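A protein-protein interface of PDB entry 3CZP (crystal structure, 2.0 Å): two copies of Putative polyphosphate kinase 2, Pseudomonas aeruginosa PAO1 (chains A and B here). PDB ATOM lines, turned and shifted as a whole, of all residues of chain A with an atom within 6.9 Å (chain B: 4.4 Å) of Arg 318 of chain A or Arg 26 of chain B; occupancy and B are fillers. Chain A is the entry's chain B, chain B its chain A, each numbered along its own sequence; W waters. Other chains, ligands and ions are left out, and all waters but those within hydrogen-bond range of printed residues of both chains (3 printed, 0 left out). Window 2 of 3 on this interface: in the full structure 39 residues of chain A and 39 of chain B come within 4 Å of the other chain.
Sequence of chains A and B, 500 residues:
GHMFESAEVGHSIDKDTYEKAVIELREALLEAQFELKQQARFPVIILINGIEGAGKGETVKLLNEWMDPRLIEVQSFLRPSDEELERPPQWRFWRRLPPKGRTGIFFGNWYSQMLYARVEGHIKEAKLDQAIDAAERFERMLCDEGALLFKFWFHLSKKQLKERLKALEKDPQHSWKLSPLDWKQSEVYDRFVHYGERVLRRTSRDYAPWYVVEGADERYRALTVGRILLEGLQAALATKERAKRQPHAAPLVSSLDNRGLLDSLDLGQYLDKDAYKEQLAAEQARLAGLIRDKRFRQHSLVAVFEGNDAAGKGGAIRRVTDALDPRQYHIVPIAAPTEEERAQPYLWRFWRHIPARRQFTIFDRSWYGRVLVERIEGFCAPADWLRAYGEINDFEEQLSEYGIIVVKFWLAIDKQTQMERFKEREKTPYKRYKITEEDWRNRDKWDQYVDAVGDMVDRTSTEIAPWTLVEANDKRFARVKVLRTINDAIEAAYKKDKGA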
ATOM      1  N   GLN A 284      -3.713  25.336   6.551  1.00  0.00           N
ATOM      2  CA  GLN A 284      -4.585  25.901   5.506  1.00  0.00           C
ATOM      3  C   GLN A 284      -5.151  27.266   5.903  1.00  0.00           C
ATOM      4  O   GLN A 284      -5.044  28.196   5.115  1.00  0.00           O
ATOM      5  CB  GLN A 284      -5.671  24.928   5.147  1.00  0.00           C
ATOM      6  CG  GLN A 284      -5.204  23.774   4.264  1.00  0.00           C
ATOM      7  CD  GLN A 284      -6.271  22.758   4.068  1.00  0.00           C
ATOM      8  OE1 GLN A 284      -7.214  22.620   4.908  1.00  0.00           O
ATOM      9  NE2 GLN A 284      -6.187  22.053   2.951  1.00  0.00           N
ATOM     10  N   LYS A 313       2.895  14.572  -5.608  1.00  0.00           N
ATOM     11  CA  LYS A 313       3.038  15.995  -5.859  1.00  0.00           C
ATOM     12  C   LYS A 313       1.692  16.667  -6.126  1.00  0.00           C
ATOM     13  O   LYS A 313       1.381  17.733  -5.601  1.00  0.00           O
ATOM     14  CB  LYS A 313       3.977  16.237  -7.086  1.00  0.00           C
ATOM     15  CG  LYS A 313       5.493  16.378  -6.752  1.00  0.00           C
ATOM     16  CD  LYS A 313       6.323  15.193  -7.193  1.00  0.00           C
ATOM     17  CE  LYS A 313       6.372  15.110  -8.716  1.00  0.00           C
ATOM     18  NZ  LYS A 313       6.518  13.708  -9.148  1.00  0.00           N
ATOM     19  N   GLY A 314       0.887  16.036  -6.967  1.00  0.00           N
ATOM     20  CA  GLY A 314      -0.457  16.518  -7.257  1.00  0.00           C
ATOM     21  C   GLY A 314      -1.337  16.659  -6.051  1.00  0.00           C
ATOM     22  O   GLY A 314      -2.050  17.632  -5.958  1.00  0.00           O
ATOM     23  N   GLY A 315      -1.319  15.675  -5.148  1.00  0.00           N
ATOM     24  CA  GLY A 315      -2.114  15.745  -3.921  1.00  0.00           C
ATOM     25  C   GLY A 315      -1.597  16.812  -2.943  1.00  0.00           C
ATOM     26  O   GLY A 315      -2.375  17.472  -2.273  1.00  0.00           O
ATOM     27  N   ALA A 316      -0.288  17.001  -2.901  1.00  0.00           N
ATOM     28  CA  ALA A 316       0.340  18.087  -2.120  1.00  0.00           C
ATOM     29  C   ALA A 316      -0.011  19.486  -2.666  1.00  0.00           C
ATOM     30  O   ALA A 316      -0.420  20.413  -1.904  1.00  0.00           O
ATOM     31  CB  ALA A 316       1.839  17.844  -2.026  1.00  0.00           C
ATOM     32  N   ILE A 317       0.054  19.639  -3.985  1.00  0.00           N
ATOM     33  CA  ILE A 317      -0.442  20.846  -4.629  1.00  0.00           C
ATOM     34  C   ILE A 317      -1.937  21.043  -4.289  1.00  0.00           C
ATOM     35  O   ILE A 317      -2.294  22.105  -3.930  1.00  0.00           O
ATOM     36  CB  ILE A 317      -0.218  20.840  -6.195  1.00  0.00           C
ATOM     37  CG1 ILE A 317       1.285  20.946  -6.523  1.00  0.00           C
ATOM     38  CG2 ILE A 317      -1.025  21.961  -6.915  1.00  0.00           C
ATOM     39  CD1 ILE A 317       1.660  20.505  -7.916  1.00  0.00           C
ATOM     40  N   ARG A 318      -2.793  20.024  -4.399  1.00  0.00           N
ATOM     41  CA  ARG A 318      -4.219  20.250  -4.122  1.00  0.00           C
ATOM     42  C   ARG A 318      -4.548  20.709  -2.683  1.00  0.00           C
ATOM     43  O   ARG A 318      -5.501  21.475  -2.492  1.00  0.00           O
ATOM     44  CB  ARG A 318      -5.065  19.047  -4.490  1.00  0.00           C
ATOM     45  CG  ARG A 318      -6.358  19.502  -5.213  1.00  0.00           C
ATOM     46  CD  ARG A 318      -7.510  18.604  -4.972  1.00  0.00           C
ATOM     47  NE  ARG A 318      -7.965  18.628  -3.580  1.00  0.00           N
ATOM     48  CZ  ARG A 318      -8.458  17.560  -2.945  1.00  0.00           C
ATOM     49  NH1 ARG A 318      -8.569  16.388  -3.556  1.00  0.00           N
ATOM     50  NH2 ARG A 318      -8.807  17.645  -1.681  1.00  0.00           N
ATOM     51  N   ARG A 319      -3.799  20.260  -1.671  1.00  0.00           N
ATOM     52  CA  ARG A 319      -4.051  20.728  -0.299  1.00  0.00           C
ATOM     53  C   ARG A 319      -3.653  22.185  -0.078  1.00  0.00           C
ATOM     54  O   ARG A 319      -4.202  22.867   0.859  1.00  0.00           O
ATOM     55  CB  ARG A 319      -3.402  19.821   0.774  1.00  0.00           C
ATOM     56  CG  ARG A 319      -3.774  18.351   0.800  1.00  0.00           C
ATOM     57  CD  ARG A 319      -5.170  18.128   0.341  1.00  0.00           C
ATOM     58  NE  ARG A 319      -5.712  16.755   0.385  1.00  0.00           N
ATOM     59  CZ  ARG A 319      -5.675  15.872  -0.601  1.00  0.00           C
ATOM     60  NH1 ARG A 319      -4.982  16.069  -1.702  1.00  0.00           N
ATOM     61  NH2 ARG A 319      -6.310  14.731  -0.461  1.00  0.00           N
ATOM     62  N   VAL A 320      -2.706  22.675  -0.905  1.00  0.00           N
ATOM     63  CA  VAL A 320      -2.392  24.103  -0.965  1.00  0.00           C
ATOM     64  C   VAL A 320      -3.547  24.845  -1.660  1.00  0.00           C
ATOM     65  O   VAL A 320      -4.135  25.722  -1.063  1.00  0.00           O
ATOM     66  CB  VAL A 320      -1.067  24.393  -1.693  1.00  0.00           C
ATOM     67  CG1 VAL A 320      -0.864  25.933  -1.772  1.00  0.00           C
ATOM     68  CG2 VAL A 320       0.112  23.684  -0.974  1.00  0.00           C
ATOM     69  N   THR A 321      -3.959  24.396  -2.837  1.00  0.00           N
ATOM     70  CA  THR A 321      -5.023  25.068  -3.564  1.00  0.00           C
ATOM     71  C   THR A 321      -6.381  25.035  -2.774  1.00  0.00           C
ATOM     72  O   THR A 321      -7.191  25.994  -2.822  1.00  0.00           O
ATOM     73  CB  THR A 321      -5.122  24.574  -5.021  1.00  0.00           C
ATOM     74  OG1 THR A 321      -5.405  23.197  -5.087  1.00  0.00           O
ATOM     75  CG2 THR A 321      -3.834  24.847  -5.802  1.00  0.00           C
ATOM     76  N   ASP A 322      -6.583  23.959  -2.021  1.00  0.00           N
ATOM     77  CA  ASP A 322      -7.758  23.792  -1.190  1.00  0.00           C
ATOM     78  C   ASP A 322      -7.911  24.963  -0.195  1.00  0.00           C
ATOM     79  O   ASP A 322      -9.021  25.303   0.186  1.00  0.00           O
ATOM     80  CB  ASP A 322      -7.702  22.462  -0.433  1.00  0.00           C
ATOM     81  CG  ASP A 322      -8.130  21.241  -1.276  1.00  0.00           C
ATOM     82  OD1 ASP A 322      -8.619  21.381  -2.416  1.00  0.00           O
ATOM     83  OD2 ASP A 322      -8.021  20.128  -0.720  1.00  0.00           O
ATOM     84  N   ALA A 323      -6.790  25.581   0.190  1.00  0.00           N
ATOM     85  CA  ALA A 323      -6.760  26.686   1.170  1.00  0.00           C
ATOM     86  C   ALA A 323      -7.197  28.003   0.595  1.00  0.00           C
ATOM     87  O   ALA A 323      -7.434  28.946   1.358  1.00  0.00           O
ATOM     88  CB  ALA A 323      -5.329  26.859   1.770  1.00  0.00           C
ATOM     89  N   ILE A 331      -1.411  27.606 -11.578  1.00  0.00           N
ATOM     90  CA  ILE A 331      -0.636  26.396 -11.635  1.00  0.00           C
ATOM     91  C   ILE A 331      -0.160  26.232 -13.032  1.00  0.00           C
ATOM     92  O   ILE A 331      -0.933  26.291 -13.931  1.00  0.00           O
ATOM     93  CB  ILE A 331      -1.419  25.151 -11.225  1.00  0.00           C
ATOM     94  CG1 ILE A 331      -2.029  25.351  -9.832  1.00  0.00           C
ATOM     95  CG2 ILE A 331      -0.453  23.920 -11.188  1.00  0.00           C
ATOM     96  CD1 ILE A 331      -2.873  24.168  -9.303  1.00  0.00           C
ATOM     97  N   ARG A 432      -6.388   7.739 -15.735  1.00  0.00           N
ATOM     98  CA  ARG A 432      -5.450   8.748 -15.253  1.00  0.00           C
ATOM     99  C   ARG A 432      -4.295   8.144 -14.449  1.00  0.00           C
ATOM    100  O   ARG A 432      -3.187   8.680 -14.447  1.00  0.00           O
ATOM    101  CB  ARG A 432      -6.180   9.798 -14.412  1.00  0.00           C
ATOM    102  CG  ARG A 432      -6.872   9.236 -13.181  1.00  0.00           C
ATOM    103  CD  ARG A 432      -7.827  10.250 -12.573  1.00  0.00           C
ATOM    104  NE  ARG A 432      -7.788  10.231 -11.113  1.00  0.00           N
ATOM    105  CZ  ARG A 432      -8.719   9.669 -10.350  1.00  0.00           C
ATOM    106  NH1 ARG A 432      -9.766   9.075 -10.904  1.00  0.00           N
ATOM    107  NH2 ARG A 432      -8.602   9.699  -9.028  1.00  0.00           N
ATOM    108  N   VAL B  22     -21.448  12.927  -5.181  1.00  0.00           N
ATOM    109  CA  VAL B  22     -20.153  13.571  -5.327  1.00  0.00           C
ATOM    110  C   VAL B  22     -18.978  12.603  -5.440  1.00  0.00           C
ATOM    111  O   VAL B  22     -18.049  12.905  -6.140  1.00  0.00           O
ATOM    112  CB  VAL B  22     -19.882  14.577  -4.175  1.00  0.00           C
ATOM    113  CG1 VAL B  22     -18.443  15.048  -4.168  1.00  0.00           C
ATOM    114  CG2 VAL B  22     -20.802  15.696  -4.319  1.00  0.00           C
ATOM    115  N   ILE B  23     -19.013  11.470  -4.752  1.00  0.00           N
ATOM    116  CA  ILE B  23     -17.912  10.526  -4.786  1.00  0.00           C
ATOM    117  C   ILE B  23     -17.728  10.047  -6.200  1.00  0.00           C
ATOM    118  O   ILE B  23     -16.620  10.029  -6.708  1.00  0.00           O
ATOM    119  CB  ILE B  23     -18.142   9.270  -3.843  1.00  0.00           C
ATOM    120  CG1 ILE B  23     -18.189   9.677  -2.371  1.00  0.00           C
ATOM    121  CG2 ILE B  23     -17.041   8.198  -4.044  1.00  0.00           C
ATOM    122  CD1 ILE B  23     -18.633   8.527  -1.450  1.00  0.00           C
ATOM    123  N   GLU B  24     -18.846   9.711  -6.840  1.00  0.00           N
ATOM    124  CA  GLU B  24     -18.854   9.221  -8.212  1.00  0.00           C
ATOM    125  C   GLU B  24     -18.508  10.353  -9.188  1.00  0.00           C
ATOM    126  O   GLU B  24     -17.719  10.136 -10.083  1.00  0.00           O
ATOM    127  CB  GLU B  24     -20.238   8.660  -8.507  1.00  0.00           C
ATOM    128  CG  GLU B  24     -20.481   7.909  -9.804  1.00  0.00           C
ATOM    129  CD  GLU B  24     -21.906   7.250  -9.764  1.00  0.00           C
ATOM    130  OE1 GLU B  24     -22.909   8.005  -9.771  1.00  0.00           O
ATOM    131  OE2 GLU B  24     -22.016   5.994  -9.658  1.00  0.00           O
ATOM    132  N   LEU B  25     -19.103  11.524  -8.973  1.00  0.00           N
ATOM    133  CA  LEU B  25     -19.038  12.654  -9.868  1.00  0.00           C
ATOM    134  C   LEU B  25     -17.617  13.121  -9.956  1.00  0.00           C
ATOM    135  O   LEU B  25     -17.149  13.396 -11.028  1.00  0.00           O
ATOM    136  CB  LEU B  25     -19.925  13.828  -9.398  1.00  0.00           C
ATOM    137  CG  LEU B  25     -19.883  15.143 -10.240  1.00  0.00           C
ATOM    138  CD1 LEU B  25     -20.235  14.893 -11.683  1.00  0.00           C
ATOM    139  CD2 LEU B  25     -20.825  16.165  -9.667  1.00  0.00           C
ATOM    140  N   ARG B  26     -16.935  13.241  -8.822  1.00  0.00           N
ATOM    141  CA  ARG B  26     -15.576  13.749  -8.839  1.00  0.00           C
ATOM    142  C   ARG B  26     -14.616  12.769  -9.532  1.00  0.00           C
ATOM    143  O   ARG B  26     -13.757  13.169 -10.347  1.00  0.00           O
ATOM    144  CB  ARG B  26     -15.134  14.235  -7.446  1.00  0.00           C
ATOM    145  CG  ARG B  26     -14.835  13.245  -6.452  1.00  0.00           C
ATOM    146  CD  ARG B  26     -14.736  13.918  -5.040  1.00  0.00           C
ATOM    147  NE  ARG B  26     -13.610  14.814  -4.847  1.00  0.00           N
ATOM    148  CZ  ARG B  26     -13.386  15.481  -3.727  1.00  0.00           C
ATOM    149  NH1 ARG B  26     -12.343  16.256  -3.648  1.00  0.00           N
ATOM    150  NH2 ARG B  26     -14.168  15.340  -2.661  1.00  0.00           N
ATOM    151  N   GLU B  27     -14.818  11.479  -9.334  1.00  0.00           N
ATOM    152  CA  GLU B  27     -13.999  10.524 -10.058  1.00  0.00           C
ATOM    153  C   GLU B  27     -14.251  10.610 -11.602  1.00  0.00           C
ATOM    154  O   GLU B  27     -13.303  10.647 -12.373  1.00  0.00           O
ATOM    155  CB  GLU B  27     -14.186   9.115  -9.514  1.00  0.00           C
ATOM    156  CG  GLU B  27     -12.892   8.406  -9.351  1.00  0.00           C
ATOM    157  CD  GLU B  27     -11.929   9.003  -8.248  1.00  0.00           C
ATOM    158  OE1 GLU B  27     -10.720   8.795  -8.439  1.00  0.00           O
ATOM    159  OE2 GLU B  27     -12.340   9.631  -7.209  1.00  0.00           O
ATOM    160  N   ALA B  28     -15.520  10.657 -12.021  1.00  0.00           N
ATOM    161  CA  ALA B  28     -15.898  10.802 -13.419  1.00  0.00           C
ATOM    162  C   ALA B  28     -15.392  12.138 -13.997  1.00  0.00           C
ATOM    163  O   ALA B  28     -14.918  12.156 -15.122  1.00  0.00           O
ATOM    164  CB  ALA B  28     -17.432  10.692 -13.624  1.00  0.00           C
ATOM    165  N   LEU B  29     -15.434  13.230 -13.217  1.00  0.00           N
ATOM    166  CA  LEU B  29     -14.857  14.496 -13.695  1.00  0.00           C
ATOM    167  C   LEU B  29     -13.350  14.411 -13.947  1.00  0.00           C
ATOM    168  O   LEU B  29     -12.843  14.752 -15.044  1.00  0.00           O
ATOM    169  CB  LEU B  29     -15.204  15.690 -12.774  1.00  0.00           C
ATOM    170  CG  LEU B  29     -16.644  16.209 -12.881  1.00  0.00           C
ATOM    171  CD1 LEU B  29     -17.058  17.141 -11.624  1.00  0.00           C
ATOM    172  CD2 LEU B  29     -16.882  16.952 -14.175  1.00  0.00           C
ATOM    173  N   LEU B  30     -12.644  13.891 -12.963  1.00  0.00           N
ATOM    174  CA  LEU B  30     -11.235  13.716 -13.061  1.00  0.00           C
ATOM    175  C   LEU B  30     -10.848  12.884 -14.276  1.00  0.00           C
ATOM    176  O   LEU B  30      -9.895  13.231 -15.006  1.00  0.00           O
ATOM    177  CB  LEU B  30     -10.683  13.114 -11.781  1.00  0.00           C
ATOM    178  CG  LEU B  30     -10.415  13.946 -10.547  1.00  0.00           C
ATOM    179  CD1 LEU B  30      -9.937  12.959  -9.427  1.00  0.00           C
ATOM    180  CD2 LEU B  30      -9.435  15.063 -10.831  1.00  0.00           C
ATOM    181  N   ASN B  64     -12.534  23.060  -8.344  1.00  0.00           N
ATOM    182  CA  ASN B  64     -11.062  22.947  -8.268  1.00  0.00           C
ATOM    183  C   ASN B  64     -10.577  22.067  -7.154  1.00  0.00           C
ATOM    184  O   ASN B  64      -9.371  21.860  -7.008  1.00  0.00           O
ATOM    185  CB  ASN B  64     -10.486  24.339  -8.165  1.00  0.00           C
ATOM    186  CG  ASN B  64     -10.414  25.031  -9.516  1.00  0.00           C
ATOM    187  OD1 ASN B  64      -9.427  24.842 -10.225  1.00  0.00           O
ATOM    188  ND2 ASN B  64     -11.479  25.831  -9.900  1.00  0.00           N
ATOM    189  N   GLU B  65     -11.520  21.544  -6.365  1.00  0.00           N
ATOM    190  CA  GLU B  65     -11.249  20.492  -5.389  1.00  0.00           C
ATOM    191  C   GLU B  65     -11.647  19.169  -5.955  1.00  0.00           C
ATOM    192  O   GLU B  65     -10.916  18.211  -5.844  1.00  0.00           O
ATOM    193  CB  GLU B  65     -12.002  20.743  -4.086  1.00  0.00           C
ATOM    194  CG  GLU B  65     -11.640  19.690  -3.035  1.00  0.00           C
ATOM    195  CD  GLU B  65     -12.282  19.995  -1.688  1.00  0.00           C
ATOM    196  OE1 GLU B  65     -12.682  21.166  -1.529  1.00  0.00           O
ATOM    197  OE2 GLU B  65     -12.351  19.046  -0.841  1.00  0.00           O
ATOM    198  N   TRP B  66     -12.768  19.149  -6.657  1.00  0.00           N
ATOM    199  CA  TRP B  66     -13.253  17.953  -7.344  1.00  0.00           C
ATOM    200  C   TRP B  66     -12.379  17.561  -8.508  1.00  0.00           C
ATOM    201  O   TRP B  66     -12.113  16.375  -8.712  1.00  0.00           O
ATOM    202  CB  TRP B  66     -14.674  18.183  -7.866  1.00  0.00           C
ATOM    203  CG  TRP B  66     -15.718  18.260  -6.749  1.00  0.00           C
ATOM    204  CD1 TRP B  66     -15.523  18.031  -5.438  1.00  0.00           C
ATOM    205  CD2 TRP B  66     -17.095  18.608  -6.900  1.00  0.00           C
ATOM    206  NE1 TRP B  66     -16.695  18.183  -4.740  1.00  0.00           N
ATOM    207  CE2 TRP B  66     -17.684  18.559  -5.614  1.00  0.00           C
ATOM    208  CE3 TRP B  66     -17.893  18.960  -7.996  1.00  0.00           C
ATOM    209  CZ2 TRP B  66     -19.047  18.823  -5.395  1.00  0.00           C
ATOM    210  CZ3 TRP B  66     -19.242  19.229  -7.777  1.00  0.00           C
ATOM    211  CH2 TRP B  66     -19.807  19.170  -6.479  1.00  0.00           C
ATOM    212  N   PRO B  69      -6.878  21.108 -10.372  1.00  0.00           N
ATOM    213  CA  PRO B  69      -6.623  22.489 -10.701  1.00  0.00           C
ATOM    214  C   PRO B  69      -5.382  22.715 -11.577  1.00  0.00           C
ATOM    215  O   PRO B  69      -5.230  23.799 -12.141  1.00  0.00           O
ATOM    216  CB  PRO B  69      -6.402  23.122  -9.330  1.00  0.00           C
ATOM    217  CG  PRO B  69      -5.881  22.007  -8.455  1.00  0.00           C
ATOM    218  CD  PRO B  69      -6.611  20.804  -8.947  1.00  0.00           C
HETATM  219  O   HOH W   1      -8.261  22.862  -4.700  1.00  0.00           O
HETATM  220  O   HOH W   2      -8.887  16.305  -6.501  1.00  0.00           O
HETATM  221  O   HOH W   3      -3.584  25.746 -14.456  1.00  0.00           O
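No position is printed for both chains.
Hydrophobic or aromatic side chains of chain B within 4 Å of the printed part of chain A: Leu 30 and Pro 69.
Printed residues of chain A that touch a printed residue of chain B: Arg 318, Thr 321, Asp 322, Ile 331 and Arg 432.
Among the printed residues, 8 pairs touch across the chains.
NH1 of Arg 432 of chain A lies within salt-bridge range of OE1 of Glu 27 of chain B (2.7 Å).
The guanidinium group (NH2) of Arg 318 of chain A lies within salt-bridge range of the side-chain carboxylate (OE2) of Glu 65 of chain B, at 3.9 Å.
Of chain B, only Arg 26 (3.8 Å), Glu 65 (3.5 Å) and Pro 69 (3.96 Å) come within 4 Å of Arg 318 of chain A.
Of the printed residues of chain B, Thr 321 of chain A touches Pro 69.
Ala 28 of chain B touches none of the printed residues of chain A.
Of the printed residues of chain A, Leu 30 of chain B touches Arg 432 (3.5 Å).
The nearest residue of chain A that does not touch Arg 26 of chain B is Arg 432 of chain A (5.7 Å).
The nearest printed residue of chain A that does not touch Pro 69 of chain B is Ile 317 of chain A (5.1 Å).
Water W1 lies within hydrogen-bond range of the side-chain carboxylate of Asp 322 of chain A (2.7 Å), the backbone carbonyl oxygen of Asn 64 of chain B (2.8 Å) and the side-chain hydroxyl of Thr 321 of chain A (2.9 Å).
Water W3 bridges the backbone carbonyl oxygen (O) of Ile 331 of chain A (2.8 Å) and the backbone carbonyl oxygen (O) of Pro 69 of chain B (3.4 Å).
Water W2 bridges O of Glu 65 of chain B (2.9 Å) and NH1 of Arg 318 of chain A (3.0 Å).
The backbone carbonyl oxygen (O) of Arg 318 of chain A sits at hydrogen-bond distance from the side-chain hydroxyl (OG1) of Thr 321 of chain A, at 3.1 Å.
NH2 of Arg 318 of chain A is in salt-bridge range of OD2 of Asp 322 of chain A, at 2.8 Å.
The guanidinium group (NH1) of Arg 26 of chain B lies within salt-bridge range of the side-chain carboxylate (OE2) of Glu 65 of chain B (3.96 Å).
The backbone carbonyl oxygen (O) of Ile 317 of chain A lies within hydrogen-bond range of the side-chain hydroxyl (OG1) of Thr 321 of chain A (3.5 Å).
NH1 of Arg 26 of chain B touches NH1 of Arg 318 of chain A (3.8 Å).
Arg 318 of chain A touches Pro 69 of chain B (CG to CD, 3.96 Å).
Thr 321 of chain A touches Pro 69 of chain B (OG1 to CG, 3.6 Å).
Glu 65 of chain B touches Asp 322 of chain A (CG to OD1, 3.5 Å).
CD1 of Ile 331 of chain A touches CB of Pro 69 of chain B, 3.7 Å away.
Leu 30 of chain B touches Arg 432 of chain A (CD1 to NH2, 3.5 Å).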
